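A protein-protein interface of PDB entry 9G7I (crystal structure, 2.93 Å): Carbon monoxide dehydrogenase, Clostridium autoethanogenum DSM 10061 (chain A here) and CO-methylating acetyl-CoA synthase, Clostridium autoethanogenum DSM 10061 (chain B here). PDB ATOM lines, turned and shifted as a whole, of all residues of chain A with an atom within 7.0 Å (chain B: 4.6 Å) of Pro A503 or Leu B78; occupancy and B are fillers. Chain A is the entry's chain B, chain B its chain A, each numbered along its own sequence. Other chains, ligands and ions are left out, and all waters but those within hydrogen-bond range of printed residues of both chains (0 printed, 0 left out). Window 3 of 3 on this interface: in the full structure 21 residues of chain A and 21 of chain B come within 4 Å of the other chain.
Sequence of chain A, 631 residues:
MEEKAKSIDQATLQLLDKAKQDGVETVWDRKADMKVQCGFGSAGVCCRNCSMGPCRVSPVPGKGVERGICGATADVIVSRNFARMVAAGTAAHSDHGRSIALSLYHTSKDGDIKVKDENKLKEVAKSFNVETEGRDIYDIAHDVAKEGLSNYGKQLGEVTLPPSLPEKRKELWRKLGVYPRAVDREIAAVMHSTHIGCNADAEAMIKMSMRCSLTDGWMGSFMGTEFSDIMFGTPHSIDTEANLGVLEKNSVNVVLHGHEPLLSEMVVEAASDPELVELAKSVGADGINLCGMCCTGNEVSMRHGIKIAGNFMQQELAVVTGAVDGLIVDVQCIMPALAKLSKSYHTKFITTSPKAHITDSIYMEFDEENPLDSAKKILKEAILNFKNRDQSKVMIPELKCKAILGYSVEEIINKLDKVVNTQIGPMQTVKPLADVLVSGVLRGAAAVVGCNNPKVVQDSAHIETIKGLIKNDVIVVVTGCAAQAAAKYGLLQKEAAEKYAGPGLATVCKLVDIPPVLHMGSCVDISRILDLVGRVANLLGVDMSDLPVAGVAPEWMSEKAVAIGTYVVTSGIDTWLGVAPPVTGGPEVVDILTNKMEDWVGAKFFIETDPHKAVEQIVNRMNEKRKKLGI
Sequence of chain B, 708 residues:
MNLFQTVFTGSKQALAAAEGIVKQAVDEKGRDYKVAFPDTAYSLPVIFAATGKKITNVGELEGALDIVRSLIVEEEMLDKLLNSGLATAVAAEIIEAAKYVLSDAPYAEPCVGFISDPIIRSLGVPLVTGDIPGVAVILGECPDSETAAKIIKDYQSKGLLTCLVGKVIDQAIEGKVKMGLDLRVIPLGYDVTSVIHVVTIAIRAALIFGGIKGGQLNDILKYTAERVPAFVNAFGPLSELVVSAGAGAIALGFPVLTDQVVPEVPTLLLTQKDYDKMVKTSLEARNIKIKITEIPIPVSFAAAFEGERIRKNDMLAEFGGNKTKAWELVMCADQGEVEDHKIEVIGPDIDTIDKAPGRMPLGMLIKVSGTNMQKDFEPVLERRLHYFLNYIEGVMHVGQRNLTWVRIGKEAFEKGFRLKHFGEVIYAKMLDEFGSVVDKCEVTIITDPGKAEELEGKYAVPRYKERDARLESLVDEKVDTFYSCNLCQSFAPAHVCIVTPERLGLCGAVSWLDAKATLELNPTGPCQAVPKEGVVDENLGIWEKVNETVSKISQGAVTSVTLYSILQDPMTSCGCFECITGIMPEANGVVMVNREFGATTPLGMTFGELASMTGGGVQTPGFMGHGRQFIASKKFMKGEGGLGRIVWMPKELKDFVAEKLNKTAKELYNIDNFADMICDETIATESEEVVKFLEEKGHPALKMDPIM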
ATOM      1  N   GLY A 440     -11.331  29.855   5.744  1.00  0.00           N
ATOM      2  CA  GLY A 440     -10.125  29.417   5.015  1.00  0.00           C
ATOM      3  C   GLY A 440     -10.350  28.108   4.279  1.00  0.00           C
ATOM      4  O   GLY A 440      -9.440  27.691   3.538  1.00  0.00           O
ATOM      5  N   VAL A 441     -11.513  27.480   4.473  1.00  0.00           N
ATOM      6  CA  VAL A 441     -11.836  26.234   3.716  1.00  0.00           C
ATOM      7  C   VAL A 441     -11.786  26.583   2.228  1.00  0.00           C
ATOM      8  O   VAL A 441     -11.133  25.838   1.472  1.00  0.00           O
ATOM      9  CB  VAL A 441     -13.209  25.670   4.122  1.00  0.00           C
ATOM     10  CG1 VAL A 441     -13.628  24.508   3.235  1.00  0.00           C
ATOM     11  CG2 VAL A 441     -13.241  25.266   5.588  1.00  0.00           C
ATOM     12  N   ARG A 443     -10.176  29.081  -0.233  1.00  0.00           N
ATOM     13  CA  ARG A 443      -9.097  30.112  -0.203  1.00  0.00           C
ATOM     14  C   ARG A 443      -9.527  31.397  -0.922  1.00  0.00           C
ATOM     15  O   ARG A 443      -8.864  32.429  -0.709  1.00  0.00           O
ATOM     16  CB  ARG A 443      -7.816  29.539  -0.816  1.00  0.00           C
ATOM     17  CG  ARG A 443      -7.559  28.081  -0.463  1.00  0.00           C
ATOM     18  CD  ARG A 443      -7.108  27.914   0.975  1.00  0.00           C
ATOM     19  NE  ARG A 443      -6.274  29.021   1.420  1.00  0.00           N
ATOM     20  CZ  ARG A 443      -6.345  29.580   2.621  1.00  0.00           C
ATOM     21  NH1 ARG A 443      -7.037  28.996   3.582  1.00  0.00           N
ATOM     22  NH2 ARG A 443      -5.722  30.722   2.859  1.00  0.00           N
ATOM     23  N   ILE A 470      -9.626  25.453  -9.105  1.00  0.00           N
ATOM     24  CA  ILE A 470     -10.431  24.566  -8.262  1.00  0.00           C
ATOM     25  C   ILE A 470      -9.530  23.605  -7.472  1.00  0.00           C
ATOM     26  O   ILE A 470      -9.841  23.295  -6.323  1.00  0.00           O
ATOM     27  CB  ILE A 470     -11.577  23.838  -9.034  1.00  0.00           C
ATOM     28  CG1 ILE A 470     -11.060  23.026 -10.232  1.00  0.00           C
ATOM     29  CG2 ILE A 470     -12.642  24.839  -9.483  1.00  0.00           C
ATOM     30  CD1 ILE A 470     -12.072  22.057 -10.796  1.00  0.00           C
ATOM     31  N   LYS A 471      -8.422  23.154  -8.063  1.00  0.00           N
ATOM     32  CA  LYS A 471      -7.491  22.276  -7.302  1.00  0.00           C
ATOM     33  C   LYS A 471      -6.966  23.023  -6.072  1.00  0.00           C
ATOM     34  O   LYS A 471      -6.825  22.383  -5.015  1.00  0.00           O
ATOM     35  CB  LYS A 471      -6.329  21.794  -8.175  1.00  0.00           C
ATOM     36  CG  LYS A 471      -5.631  20.540  -7.662  1.00  0.00           C
ATOM     37  CD  LYS A 471      -6.442  19.273  -7.796  1.00  0.00           C
ATOM     38  CE  LYS A 471      -5.651  18.046  -7.397  1.00  0.00           C
ATOM     39  NZ  LYS A 471      -6.539  16.933  -6.986  1.00  0.00           N
ATOM     40  N   ASN A 472      -6.686  24.321  -6.208  1.00  0.00           N
ATOM     41  CA  ASN A 472      -6.148  25.098  -5.097  1.00  0.00           C
ATOM     42  C   ASN A 472      -7.278  25.643  -4.205  1.00  0.00           C
ATOM     43  O   ASN A 472      -7.139  26.722  -3.634  1.00  0.00           O
ATOM     44  CB  ASN A 472      -5.283  26.244  -5.630  1.00  0.00           C
ATOM     45  CG  ASN A 472      -3.934  25.781  -6.116  1.00  0.00           C
ATOM     46  OD1 ASN A 472      -2.927  25.899  -5.417  1.00  0.00           O
ATOM     47  ND2 ASN A 472      -3.874  25.232  -7.315  1.00  0.00           N
ATOM     48  N   ASP A 473      -8.379  24.890  -4.061  1.00  0.00           N
ATOM     49  CA  ASP A 473      -9.521  25.271  -3.226  1.00  0.00           C
ATOM     50  C   ASP A 473     -10.106  26.674  -3.485  1.00  0.00           C
ATOM     51  O   ASP A 473     -10.567  27.321  -2.548  1.00  0.00           O
ATOM     52  CB  ASP A 473      -9.140  25.104  -1.743  1.00  0.00           C
ATOM     53  CG  ASP A 473      -9.146  23.670  -1.262  1.00  0.00           C
ATOM     54  OD1 ASP A 473      -9.857  22.843  -1.871  1.00  0.00           O
ATOM     55  OD2 ASP A 473      -8.464  23.376  -0.256  1.00  0.00           O
ATOM     56  N   GLU A 498     -14.921  15.645  -6.930  1.00  0.00           N
ATOM     57  CA  GLU A 498     -13.990  14.634  -6.442  1.00  0.00           C
ATOM     58  C   GLU A 498     -12.837  14.440  -7.408  1.00  0.00           C
ATOM     59  O   GLU A 498     -11.727  14.162  -6.968  1.00  0.00           O
ATOM     60  CB  GLU A 498     -14.695  13.291  -6.200  1.00  0.00           C
ATOM     61  CG  GLU A 498     -15.544  13.265  -4.940  1.00  0.00           C
ATOM     62  CD  GLU A 498     -14.788  13.542  -3.652  1.00  0.00           C
ATOM     63  OE1 GLU A 498     -13.870  12.757  -3.319  1.00  0.00           O
ATOM     64  OE2 GLU A 498     -15.116  14.544  -2.973  1.00  0.00           O
ATOM     65  N   ALA A 501     -11.329  18.988  -7.787  1.00  0.00           N
ATOM     66  CA  ALA A 501     -11.275  20.011  -6.736  1.00  0.00           C
ATOM     67  C   ALA A 501     -10.412  19.630  -5.530  1.00  0.00           C
ATOM     68  O   ALA A 501     -10.242  18.448  -5.229  1.00  0.00           O
ATOM     69  CB  ALA A 501     -12.680  20.367  -6.284  1.00  0.00           C
ATOM     70  N   GLY A 502      -9.887  20.649  -4.848  1.00  0.00           N
ATOM     71  CA  GLY A 502      -9.041  20.477  -3.677  1.00  0.00           C
ATOM     72  C   GLY A 502      -9.786  19.955  -2.463  1.00  0.00           C
ATOM     73  O   GLY A 502     -10.979  19.668  -2.547  1.00  0.00           O
ATOM     74  N   PRO A 503      -9.149  19.828  -1.277  1.00  0.00           N
ATOM     75  CA  PRO A 503      -9.828  19.243  -0.117  1.00  0.00           C
ATOM     76  C   PRO A 503     -11.002  20.112   0.350  1.00  0.00           C
ATOM     77  O   PRO A 503     -12.082  19.580   0.524  1.00  0.00           O
ATOM     78  CB  PRO A 503      -8.736  19.213   0.963  1.00  0.00           C
ATOM     79  CG  PRO A 503      -7.765  20.292   0.545  1.00  0.00           C
ATOM     80  CD  PRO A 503      -7.776  20.244  -0.968  1.00  0.00           C
ATOM     81  N   GLY A 504     -10.771  21.413   0.534  1.00  0.00           N
ATOM     82  CA  GLY A 504     -11.804  22.322   1.009  1.00  0.00           C
ATOM     83  C   GLY A 504     -12.965  22.476   0.046  1.00  0.00           C
ATOM     84  O   GLY A 504     -14.122  22.358   0.452  1.00  0.00           O
ATOM     85  N   LEU A 505     -12.674  22.738  -1.232  1.00  0.00           N
ATOM     86  CA  LEU A 505     -13.723  22.912  -2.227  1.00  0.00           C
ATOM     87  C   LEU A 505     -14.531  21.626  -2.428  1.00  0.00           C
ATOM     88  O   LEU A 505     -15.751  21.701  -2.534  1.00  0.00           O
ATOM     89  CB  LEU A 505     -13.131  23.423  -3.549  1.00  0.00           C
ATOM     90  CG  LEU A 505     -14.096  23.602  -4.728  1.00  0.00           C
ATOM     91  CD1 LEU A 505     -15.193  24.620  -4.433  1.00  0.00           C
ATOM     92  CD2 LEU A 505     -13.348  24.063  -5.939  1.00  0.00           C
ATOM     93  N   ALA A 506     -13.882  20.454  -2.450  1.00  0.00           N
ATOM     94  CA  ALA A 506     -14.613  19.195  -2.605  1.00  0.00           C
ATOM     95  C   ALA A 506     -15.560  18.977  -1.421  1.00  0.00           C
ATOM     96  O   ALA A 506     -16.633  18.403  -1.591  1.00  0.00           O
ATOM     97  CB  ALA A 506     -13.647  18.033  -2.709  1.00  0.00           C
ATOM     98  N   THR A 507     -15.159  19.428  -0.228  1.00  0.00           N
ATOM     99  CA  THR A 507     -15.969  19.314   0.982  1.00  0.00           C
ATOM    100  C   THR A 507     -17.188  20.229   0.854  1.00  0.00           C
ATOM    101  O   THR A 507     -18.307  19.796   1.136  1.00  0.00           O
ATOM    102  CB  THR A 507     -15.134  19.696   2.216  1.00  0.00           C
ATOM    103  OG1 THR A 507     -14.103  18.726   2.405  1.00  0.00           O
ATOM    104  CG2 THR A 507     -15.977  19.821   3.473  1.00  0.00           C
ATOM    105  N   VAL A 508     -16.972  21.494   0.422  1.00  0.00           N
ATOM    106  CA  VAL A 508     -18.055  22.465   0.257  1.00  0.00           C
ATOM    107  C   VAL A 508     -19.031  21.971  -0.807  1.00  0.00           C
ATOM    108  O   VAL A 508     -20.239  22.091  -0.627  1.00  0.00           O
ATOM    109  CB  VAL A 508     -17.509  23.876  -0.070  1.00  0.00           C
ATOM    110  CG1 VAL A 508     -18.628  24.815  -0.507  1.00  0.00           C
ATOM    111  CG2 VAL A 508     -16.764  24.462   1.123  1.00  0.00           C
ATOM    112  N   PHE B   4      -7.136  28.566  10.858  1.00  0.00           N
ATOM    113  CA  PHE B   4      -5.988  27.701  10.606  1.00  0.00           C
ATOM    114  C   PHE B   4      -4.867  27.910  11.614  1.00  0.00           C
ATOM    115  O   PHE B   4      -4.466  26.966  12.292  1.00  0.00           O
ATOM    116  CB  PHE B   4      -5.462  27.904   9.170  1.00  0.00           C
ATOM    117  CG  PHE B   4      -6.251  27.134   8.146  1.00  0.00           C
ATOM    118  CD1 PHE B   4      -7.469  27.601   7.694  1.00  0.00           C
ATOM    119  CD2 PHE B   4      -5.826  25.892   7.717  1.00  0.00           C
ATOM    120  CE1 PHE B   4      -8.224  26.862   6.796  1.00  0.00           C
ATOM    121  CE2 PHE B   4      -6.579  25.158   6.815  1.00  0.00           C
ATOM    122  CZ  PHE B   4      -7.771  25.649   6.356  1.00  0.00           C
ATOM    123  N   MET B  77      -4.680  24.585   4.212  1.00  0.00           N
ATOM    124  CA  MET B  77      -5.555  23.778   3.321  1.00  0.00           C
ATOM    125  C   MET B  77      -6.359  22.868   4.255  1.00  0.00           C
ATOM    126  O   MET B  77      -5.771  22.403   5.248  1.00  0.00           O
ATOM    127  CB  MET B  77      -4.734  22.926   2.351  1.00  0.00           C
ATOM    128  CG  MET B  77      -4.158  23.715   1.192  1.00  0.00           C
ATOM    129  SD  MET B  77      -5.410  24.164  -0.036  1.00  0.00           S
ATOM    130  CE  MET B  77      -5.418  22.689  -1.052  1.00  0.00           C
ATOM    131  N   LEU B  78      -7.639  22.617   3.967  1.00  0.00           N
ATOM    132  CA  LEU B  78      -8.500  21.848   4.912  1.00  0.00           C
ATOM    133  C   LEU B  78      -7.778  20.611   5.459  1.00  0.00           C
ATOM    134  O   LEU B  78      -7.601  20.539   6.689  1.00  0.00           O
ATOM    135  CB  LEU B  78      -9.788  21.440   4.188  1.00  0.00           C
ATOM    136  CG  LEU B  78     -10.863  20.812   5.072  1.00  0.00           C
ATOM    137  CD1 LEU B  78     -11.024  21.597   6.365  1.00  0.00           C
ATOM    138  CD2 LEU B  78     -12.188  20.725   4.332  1.00  0.00           C
ATOM    139  N   ASP B  79      -7.393  19.671   4.593  1.00  0.00           N
ATOM    140  CA  ASP B  79      -6.768  18.401   5.054  1.00  0.00           C
ATOM    141  C   ASP B  79      -5.738  18.673   6.152  1.00  0.00           C
ATOM    142  O   ASP B  79      -5.702  17.897   7.125  1.00  0.00           O
ATOM    143  CB  ASP B  79      -6.111  17.668   3.883  1.00  0.00           C
ATOM    144  CG  ASP B  79      -4.970  18.449   3.255  1.00  0.00           C
ATOM    145  OD1 ASP B  79      -5.163  19.651   2.984  1.00  0.00           O
ATOM    146  OD2 ASP B  79      -3.898  17.850   3.044  1.00  0.00           O
ATOM    147  N   LYS B  80      -4.936  19.727   6.003  1.00  0.00           N
ATOM    148  CA  LYS B  80      -3.861  20.030   6.955  1.00  0.00           C
ATOM    149  C   LYS B  80      -4.471  20.391   8.306  1.00  0.00           C
ATOM    150  O   LYS B  80      -3.971  19.955   9.343  1.00  0.00           O
ATOM    151  CB  LYS B  80      -2.971  21.191   6.456  1.00  0.00           C
ATOM    152  CG  LYS B  80      -2.578  21.146   4.974  1.00  0.00           C
ATOM    153  CD  LYS B  80      -1.412  20.234   4.690  1.00  0.00           C
ATOM    154  CE  LYS B  80      -1.147  20.112   3.206  1.00  0.00           C
ATOM    155  NZ  LYS B  80      -1.148  18.696   2.770  1.00  0.00           N
ATOM    156  N   LEU B  81      -5.542  21.188   8.276  1.00  0.00           N
ATOM    157  CA  LEU B  81      -6.239  21.594   9.524  1.00  0.00           C
ATOM    158  C   LEU B  81      -6.761  20.339  10.224  1.00  0.00           C
ATOM    159  O   LEU B  81      -6.538  20.205  11.439  1.00  0.00           O
ATOM    160  CB  LEU B  81      -7.393  22.526   9.149  1.00  0.00           C
ATOM    161  CG  LEU B  81      -8.011  23.329  10.291  1.00  0.00           C
ATOM    162  CD1 LEU B  81      -8.373  24.731   9.822  1.00  0.00           C
ATOM    163  CD2 LEU B  81      -9.241  22.624  10.839  1.00  0.00           C
ATOM    164  N   LEU B  82      -7.435  19.462   9.479  1.00  0.00           N
ATOM    165  CA  LEU B  82      -8.009  18.269  10.094  1.00  0.00           C
ATOM    166  C   LEU B  82      -6.905  17.368  10.667  1.00  0.00           C
ATOM    167  O   LEU B  82      -7.063  16.859  11.775  1.00  0.00           O
ATOM    168  CB  LEU B  82      -8.904  17.513   9.095  1.00  0.00           C
ATOM    169  CG  LEU B  82     -10.048  18.330   8.463  1.00  0.00           C
ATOM    170  CD1 LEU B  82     -10.642  17.602   7.286  1.00  0.00           C
ATOM    171  CD2 LEU B  82     -11.142  18.633   9.462  1.00  0.00           C
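The side-chain carboxylate (OD2) of Asp A473 sits close to the side-chain sulfur (SD) of Met B77 (3.2 Å).
The side-chain carboxylate (OD2) of Asp B79 is in salt-bridge range of the side-chain amino group (NZ) of Lys B80 (2.9 Å).
The guanidinium group (NH1) of Arg A443 is in hydrogen-bond range of the backbone carbonyl oxygen (O) of Gly A440 (2.7 Å).
N of Arg A443 sits at hydrogen-bond distance from O of Asp A473, 2.9 Å away.
N of Gly A504 sits at hydrogen-bond distance from OD1 of Asp A473, 2.9 Å away.
OD1 of Asp A473 is in hydrogen-bond range of N of Leu A505, at 2.9 Å.
O of Pro A503 lies within hydrogen-bond range of OG1 of Thr A507 (2.9 Å).
Gly A440 touches Phe B4 (C to CE1, 3.5 Å).
Pro A503 touches Met B77 (CD to CE, 3.4 Å).
Pro A503 touches Leu B78.
Pro A503 touches Asp B79 (CG to OD1, 3.6 Å).
Leu B78 touches Gly A504 (CD2 to CA, 3.7 Å).
Thr A507 touches Leu B78 (OG1 to CD2, 3.4 Å).
Of the printed residues of chain A, Met B77 touches Asp A473 (3.2 Å) and Pro A503 (3.4 Å).
Printed residues of chain A within 4 Å of Asp B79: Pro A503 (3.6 Å).
Of the printed residues of chain A, Phe B4 touches Gly A440.
Printed residues of chain B within 4 Å of Gly A504: Leu B78 (3.7 Å).
Of the printed residues of chain B, Gly A440 touches Phe B4 (3.5 Å).
Arg A443 touches none of the printed residues of chain B.
The nearest printed residue of chain B that does not touch Pro A503 is Lys B80 (6.2 Å).
Hydrophobic or aromatic side chains of chain B that line the printed part of chain A: Phe B4, Met B77 and Leu B78.
Of the 16 printed residues of chain A, 5 touch a printed residue of chain B.
Hydrophobic or aromatic side chains of chain A within 4 Å of the printed part of chain B: Pro A503.
Along chain A the printed residues that touch a printed residue of chain B span positions 440 to 507.
Among the printed residues, 7 pairs touch across the chains.
Among the printed residues, no Asp or Glu carboxylate lies within 4 Å of a Lys or Arg side-chain nitrogen of the other chain.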
